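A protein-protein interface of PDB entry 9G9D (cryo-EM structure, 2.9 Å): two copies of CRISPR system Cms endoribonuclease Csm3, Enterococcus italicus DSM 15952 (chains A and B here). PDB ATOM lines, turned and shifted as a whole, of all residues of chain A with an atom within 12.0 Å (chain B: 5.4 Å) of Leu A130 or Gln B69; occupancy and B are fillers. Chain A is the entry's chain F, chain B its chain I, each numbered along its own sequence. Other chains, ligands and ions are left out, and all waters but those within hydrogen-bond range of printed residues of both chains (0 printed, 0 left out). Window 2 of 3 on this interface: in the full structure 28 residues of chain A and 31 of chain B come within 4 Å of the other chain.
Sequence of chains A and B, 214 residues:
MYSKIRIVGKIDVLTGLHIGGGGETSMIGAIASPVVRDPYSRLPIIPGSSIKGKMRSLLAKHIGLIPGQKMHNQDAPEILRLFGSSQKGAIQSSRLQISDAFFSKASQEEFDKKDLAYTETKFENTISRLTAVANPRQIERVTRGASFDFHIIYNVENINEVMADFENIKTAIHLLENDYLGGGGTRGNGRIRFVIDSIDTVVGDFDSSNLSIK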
ATOM      1  N   THR A 126      -9.057  33.694  -1.236  1.00  0.00           N
ATOM      2  CA  THR A 126      -9.909  32.538  -1.473  1.00  0.00           C
ATOM      3  C   THR A 126     -10.048  32.326  -2.970  1.00  0.00           C
ATOM      4  O   THR A 126     -10.470  33.236  -3.686  1.00  0.00           O
ATOM      5  CB  THR A 126     -11.289  32.743  -0.853  1.00  0.00           C
ATOM      6  OG1 THR A 126     -11.139  33.153   0.510  1.00  0.00           O
ATOM      7  CG2 THR A 126     -12.101  31.460  -0.910  1.00  0.00           C
ATOM      8  N   ILE A 127      -9.692  31.140  -3.440  1.00  0.00           N
ATOM      9  CA  ILE A 127      -9.791  30.802  -4.853  1.00  0.00           C
ATOM     10  C   ILE A 127     -11.125  30.098  -5.059  1.00  0.00           C
ATOM     11  O   ILE A 127     -11.379  29.039  -4.474  1.00  0.00           O
ATOM     12  CB  ILE A 127      -8.612  29.939  -5.321  1.00  0.00           C
ATOM     13  CG1 ILE A 127      -7.422  30.819  -5.711  1.00  0.00           C
ATOM     14  CG2 ILE A 127      -9.010  29.074  -6.504  1.00  0.00           C
ATOM     15  CD1 ILE A 127      -6.716  31.465  -4.553  1.00  0.00           C
ATOM     16  N   SER A 128     -11.986  30.696  -5.879  1.00  0.00           N
ATOM     17  CA  SER A 128     -13.286  30.108  -6.161  1.00  0.00           C
ATOM     18  C   SER A 128     -13.118  28.769  -6.868  1.00  0.00           C
ATOM     19  O   SER A 128     -12.125  28.524  -7.555  1.00  0.00           O
ATOM     20  CB  SER A 128     -14.121  31.060  -7.015  1.00  0.00           C
ATOM     21  OG  SER A 128     -14.274  32.311  -6.367  1.00  0.00           O
ATOM     22  N   ARG A 129     -14.097  27.890  -6.684  1.00  0.00           N
ATOM     23  CA  ARG A 129     -13.984  26.534  -7.198  1.00  0.00           C
ATOM     24  C   ARG A 129     -14.505  26.385  -8.622  1.00  0.00           C
ATOM     25  O   ARG A 129     -14.157  25.406  -9.292  1.00  0.00           O
ATOM     26  CB  ARG A 129     -14.714  25.561  -6.265  1.00  0.00           C
ATOM     27  CG  ARG A 129     -14.310  24.106  -6.445  1.00  0.00           C
ATOM     28  CD  ARG A 129     -13.871  23.476  -5.134  1.00  0.00           C
ATOM     29  NE  ARG A 129     -12.660  24.084  -4.594  1.00  0.00           N
ATOM     30  CZ  ARG A 129     -12.052  23.677  -3.488  1.00  0.00           C
ATOM     31  NH1 ARG A 129     -12.515  22.660  -2.779  1.00  0.00           N
ATOM     32  NH2 ARG A 129     -10.954  24.307  -3.082  1.00  0.00           N
ATOM     33  N   LEU A 130     -15.266  27.373  -9.106  1.00  0.00           N
ATOM     34  CA  LEU A 130     -15.852  27.293 -10.475  1.00  0.00           C
ATOM     35  C   LEU A 130     -15.231  28.370 -11.383  1.00  0.00           C
ATOM     36  O   LEU A 130     -15.133  28.119 -12.603  1.00  0.00           O
ATOM     37  CB  LEU A 130     -17.379  27.393 -10.417  1.00  0.00           C
ATOM     38  CG  LEU A 130     -17.990  28.783 -10.204  1.00  0.00           C
ATOM     39  CD1 LEU A 130     -19.493  28.703 -10.403  1.00  0.00           C
ATOM     40  CD2 LEU A 130     -17.675  29.407  -8.853  1.00  0.00           C
ATOM     41  N   THR A 131     -14.830  29.513 -10.821  1.00  0.00           N
ATOM     42  CA  THR A 131     -14.215  30.588 -11.584  1.00  0.00           C
ATOM     43  C   THR A 131     -12.710  30.686 -11.371  1.00  0.00           C
ATOM     44  O   THR A 131     -12.014  31.230 -12.234  1.00  0.00           O
ATOM     45  CB  THR A 131     -14.863  31.931 -11.221  1.00  0.00           C
ATOM     46  OG1 THR A 131     -16.282  31.763 -11.130  1.00  0.00           O
ATOM     47  CG2 THR A 131     -14.565  32.978 -12.281  1.00  0.00           C
ATOM     48  N   ALA A 132     -12.199  30.155 -10.258  1.00  0.00           N
ATOM     49  CA  ALA A 132     -10.776  30.214  -9.920  1.00  0.00           C
ATOM     50  C   ALA A 132     -10.276  31.657  -9.882  1.00  0.00           C
ATOM     51  O   ALA A 132      -9.177  31.974 -10.342  1.00  0.00           O
ATOM     52  CB  ALA A 132      -9.943  29.366 -10.883  1.00  0.00           C
ATOM     53  N   VAL A 133     -11.099  32.538  -9.323  1.00  0.00           N
ATOM     54  CA  VAL A 133     -10.769  33.948  -9.170  1.00  0.00           C
ATOM     55  C   VAL A 133     -10.481  34.210  -7.699  1.00  0.00           C
ATOM     56  O   VAL A 133     -11.253  33.799  -6.823  1.00  0.00           O
ATOM     57  CB  VAL A 133     -11.898  34.855  -9.694  1.00  0.00           C
ATOM     58  CG1 VAL A 133     -13.243  34.422  -9.136  1.00  0.00           C
ATOM     59  CG2 VAL A 133     -11.620  36.306  -9.349  1.00  0.00           C
ATOM     60  N   ALA A 134      -9.357  34.863  -7.427  1.00  0.00           N
ATOM     61  CA  ALA A 134      -8.965  35.131  -6.053  1.00  0.00           C
ATOM     62  C   ALA A 134      -9.835  36.219  -5.440  1.00  0.00           C
ATOM     63  O   ALA A 134     -10.231  37.176  -6.110  1.00  0.00           O
ATOM     64  CB  ALA A 134      -7.494  35.540  -5.991  1.00  0.00           C
ATOM     65  N   ASN A 135     -10.147  36.052  -4.159  1.00  0.00           N
ATOM     66  CA  ASN A 135     -10.801  37.073  -3.359  1.00  0.00           C
ATOM     67  C   ASN A 135      -9.883  37.415  -2.198  1.00  0.00           C
ATOM     68  O   ASN A 135      -9.631  36.545  -1.353  1.00  0.00           O
ATOM     69  CB  ASN A 135     -12.155  36.583  -2.851  1.00  0.00           C
ATOM     70  CG  ASN A 135     -12.955  37.675  -2.172  1.00  0.00           C
ATOM     71  OD1 ASN A 135     -12.738  38.862  -2.413  1.00  0.00           O
ATOM     72  ND2 ASN A 135     -13.891  37.277  -1.320  1.00  0.00           N
ATOM     73  N   GLY B  64     -13.162  14.826  -7.137  1.00  0.00           N
ATOM     74  CA  GLY B  64     -14.111  15.250  -8.150  1.00  0.00           C
ATOM     75  C   GLY B  64     -14.875  16.472  -7.682  1.00  0.00           C
ATOM     76  O   GLY B  64     -15.006  16.740  -6.488  1.00  0.00           O
ATOM     77  N   LEU B  65     -15.390  17.233  -8.642  1.00  0.00           N
ATOM     78  CA  LEU B  65     -16.188  18.417  -8.366  1.00  0.00           C
ATOM     79  C   LEU B  65     -17.542  18.277  -9.042  1.00  0.00           C
ATOM     80  O   LEU B  65     -17.622  17.850 -10.198  1.00  0.00           O
ATOM     81  CB  LEU B  65     -15.488  19.688  -8.856  1.00  0.00           C
ATOM     82  CG  LEU B  65     -14.143  20.050  -8.231  1.00  0.00           C
ATOM     83  CD1 LEU B  65     -13.639  21.355  -8.816  1.00  0.00           C
ATOM     84  CD2 LEU B  65     -14.260  20.150  -6.723  1.00  0.00           C
ATOM     85  N   ILE B  66     -18.599  18.630  -8.322  1.00  0.00           N
ATOM     86  CA  ILE B  66     -19.933  18.666  -8.932  1.00  0.00           C
ATOM     87  C   ILE B  66     -19.981  19.799  -9.950  1.00  0.00           C
ATOM     88  O   ILE B  66     -19.312  20.830  -9.752  1.00  0.00           O
ATOM     89  CB  ILE B  66     -21.006  18.842  -7.855  1.00  0.00           C
ATOM     90  CG1 ILE B  66     -20.702  20.066  -6.990  1.00  0.00           C
ATOM     91  CG2 ILE B  66     -21.106  17.590  -6.998  1.00  0.00           C
ATOM     92  CD1 ILE B  66     -21.713  20.309  -5.893  1.00  0.00           C
ATOM     93  N   PRO B  67     -20.717  19.656 -11.050  1.00  0.00           N
ATOM     94  CA  PRO B  67     -20.787  20.748 -12.028  1.00  0.00           C
ATOM     95  C   PRO B  67     -21.378  22.008 -11.411  1.00  0.00           C
ATOM     96  O   PRO B  67     -22.320  21.953 -10.619  1.00  0.00           O
ATOM     97  CB  PRO B  67     -21.686  20.180 -13.133  1.00  0.00           C
ATOM     98  CG  PRO B  67     -22.449  19.074 -12.479  1.00  0.00           C
ATOM     99  CD  PRO B  67     -21.525  18.495 -11.454  1.00  0.00           C
ATOM    100  N   GLY B  68     -20.812  23.150 -11.787  1.00  0.00           N
ATOM    101  CA  GLY B  68     -21.251  24.418 -11.225  1.00  0.00           C
ATOM    102  C   GLY B  68     -21.017  24.537  -9.735  1.00  0.00           C
ATOM    103  O   GLY B  68     -21.856  25.099  -9.020  1.00  0.00           O
ATOM    104  N   GLN B  69     -19.894  24.016  -9.247  1.00  0.00           N
ATOM    105  CA  GLN B  69     -19.576  24.027  -7.820  1.00  0.00           C
ATOM    106  C   GLN B  69     -19.132  25.430  -7.427  1.00  0.00           C
ATOM    107  O   GLN B  69     -17.976  25.809  -7.620  1.00  0.00           O
ATOM    108  CB  GLN B  69     -18.502  22.993  -7.511  1.00  0.00           C
ATOM    109  CG  GLN B  69     -18.127  22.904  -6.048  1.00  0.00           C
ATOM    110  CD  GLN B  69     -17.362  21.642  -5.736  1.00  0.00           C
ATOM    111  OE1 GLN B  69     -17.478  20.643  -6.442  1.00  0.00           O
ATOM    112  NE2 GLN B  69     -16.573  21.678  -4.673  1.00  0.00           N
ATOM    113  N   LYS B  70     -20.060  26.208  -6.871  1.00  0.00           N
ATOM    114  CA  LYS B  70     -19.779  27.604  -6.556  1.00  0.00           C
ATOM    115  C   LYS B  70     -18.989  27.755  -5.262  1.00  0.00           C
ATOM    116  O   LYS B  70     -18.141  28.647  -5.153  1.00  0.00           O
ATOM    117  CB  LYS B  70     -21.089  28.382  -6.462  1.00  0.00           C
ATOM    118  CG  LYS B  70     -22.139  27.928  -7.454  1.00  0.00           C
ATOM    119  CD  LYS B  70     -23.536  28.280  -6.975  1.00  0.00           C
ATOM    120  CE  LYS B  70     -24.595  27.575  -7.802  1.00  0.00           C
ATOM    121  NZ  LYS B  70     -24.424  26.097  -7.757  1.00  0.00           N
ATOM    122  N   MET B  71     -19.252  26.905  -4.272  1.00  0.00           N
ATOM    123  CA  MET B  71     -18.770  27.110  -2.916  1.00  0.00           C
ATOM    124  C   MET B  71     -17.785  26.021  -2.508  1.00  0.00           C
ATOM    125  O   MET B  71     -17.784  24.913  -3.048  1.00  0.00           O
ATOM    126  CB  MET B  71     -19.934  27.134  -1.916  1.00  0.00           C
ATOM    127  CG  MET B  71     -20.887  28.301  -2.082  1.00  0.00           C
ATOM    128  SD  MET B  71     -20.159  29.870  -1.582  1.00  0.00           S
ATOM    129  CE  MET B  71     -21.588  30.945  -1.663  1.00  0.00           C
ATOM    130  N   HIS B  72     -16.939  26.364  -1.533  1.00  0.00           N
ATOM    131  CA  HIS B  72     -16.090  25.361  -0.902  1.00  0.00           C
ATOM    132  C   HIS B  72     -16.894  24.453   0.016  1.00  0.00           C
ATOM    133  O   HIS B  72     -16.528  23.290   0.210  1.00  0.00           O
ATOM    134  CB  HIS B  72     -14.963  26.033  -0.118  1.00  0.00           C
ATOM    135  CG  HIS B  72     -13.981  26.768  -0.974  1.00  0.00           C
ATOM    136  ND1 HIS B  72     -12.958  26.135  -1.643  1.00  0.00           N
ATOM    137  CD2 HIS B  72     -13.861  28.085  -1.263  1.00  0.00           C
ATOM    138  CE1 HIS B  72     -12.252  27.028  -2.312  1.00  0.00           C
ATOM    139  NE2 HIS B  72     -12.780  28.220  -2.099  1.00  0.00           N
ATOM    140  N   GLN B  74     -19.581  23.191  -0.690  1.00  0.00           N
ATOM    141  CA  GLN B  74     -19.964  22.109  -1.588  1.00  0.00           C
ATOM    142  C   GLN B  74     -18.694  21.361  -1.967  1.00  0.00           C
ATOM    143  O   GLN B  74     -17.927  21.819  -2.819  1.00  0.00           O
ATOM    144  CB  GLN B  74     -20.676  22.652  -2.824  1.00  0.00           C
ATOM    145  CG  GLN B  74     -21.821  23.599  -2.526  1.00  0.00           C
ATOM    146  CD  GLN B  74     -22.482  24.115  -3.787  1.00  0.00           C
ATOM    147  OE1 GLN B  74     -22.460  23.457  -4.825  1.00  0.00           O
ATOM    148  NE2 GLN B  74     -23.068  25.303  -3.705  1.00  0.00           N
ATOM    149  N   ASP B  75     -18.462  20.222  -1.326  1.00  0.00           N
ATOM    150  CA  ASP B  75     -17.255  19.440  -1.552  1.00  0.00           C
ATOM    151  C   ASP B  75     -17.573  17.981  -1.256  1.00  0.00           C
ATOM    152  O   ASP B  75     -18.679  17.641  -0.829  1.00  0.00           O
ATOM    153  CB  ASP B  75     -16.093  19.948  -0.692  1.00  0.00           C
ATOM    154  CG  ASP B  75     -15.106  20.784  -1.479  1.00  0.00           C
ATOM    155  OD1 ASP B  75     -14.944  20.529  -2.689  1.00  0.00           O
ATOM    156  OD2 ASP B  75     -14.486  21.693  -0.891  1.00  0.00           O
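NH2 of Arg A129 sits at hydrogen-bond distance from ND1 of His B72 (3.1 Å). The side-chain carboxylate of Asp B75 lies within salt-bridge range of the guanidinium group of Arg A129, 2.9 Å away. The backbone carbonyl oxygen (O) of Ile A127 lies within hydrogen-bond range of a ring nitrogen (NE2) of His B72. The backbone NH (N) of Leu A130 sits close to the backbone carbonyl oxygen (O) of Gln B69, at 3.5 Å.
The backbone carbonyl oxygen of Thr A126 lies within hydrogen-bond range of the backbone NH of Asn A135 (2.9 Å). The side-chain amide nitrogen (NE2) of Gln B69 lies within hydrogen-bond range of the side-chain carboxylate (OD1) of Asp B75 (2.8 Å). The backbone NH (N) of Ile B66 is in hydrogen-bond range of the side-chain amide oxygen (OE1) of Gln B69 (3.0 Å). O of Gly B68 lies within hydrogen-bond range of NZ of Lys B70 (3.0 Å).
Printed residues of chain A that touch a printed residue of chain B: Thr A126, Ile A127, Arg A129 and Leu A130. Hydrophobic or aromatic side chains of chain A that line the printed part of chain B: Leu A130. Of the 11 printed residues of chain B, 5 touch a printed residue of chain A. Among the printed residues, 8 pairs touch across the chains. Among the printed residues, Asp or Glu carboxylates within 4 Å of a Lys or Arg side-chain nitrogen of the other chain: Arg A129 with Asp B75.
No position is printed for both chains. Of the 8 pairs that touch across the chains among the printed residues, none has its exchanged pair printed and touching as well.
Leu A130 touches just these residues of chain B: Gln B69 (3.3 Å) and Lys B70 (3.6 Å). Of the printed residues of chain A, Gln B69 touches Arg A129 (3.3 Å) and Leu A130 (3.3 Å). No residue of chain A comes within 4 Å of Gly B64. Leu B65 touches just one residue of chain A: Arg A129 (3.7 Å). No residue of chain A comes within 4 Å of Ile B66. Of chain A, only Leu A130 (3.6 Å) comes within 4 Å of Lys B70. No residue of chain A comes within 4 Å of Gln B74. Of the printed residues of chain A, Asp B75 touches Arg A129 (2.9 Å). Printed residues of chain B within 4 Å of Thr A126: His B72. Of the printed residues of chain B, Ile A127 touches His B72 (2.9 Å). Of the printed residues of chain B, Arg A129 touches Leu B65 (3.7 Å), Gln B69 (3.3 Å), His B72 (3.1 Å) and Asp B75 (2.9 Å). The nearest residue of chain A that does not touch Gln B69 is Ser A128 (5.7 Å). The nearest printed residue of chain B that does not touch Ile A127 is Lys B70 (6.8 Å).
Among the printed residues, merely in contact across the chains: Thr A126 with His B72 (3.5 Å), Arg A129 with Leu B65 (3.7 Å), Arg A129 with Gln B69 (3.3 Å) and Leu A130 with Lys B70 (3.6 Å).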
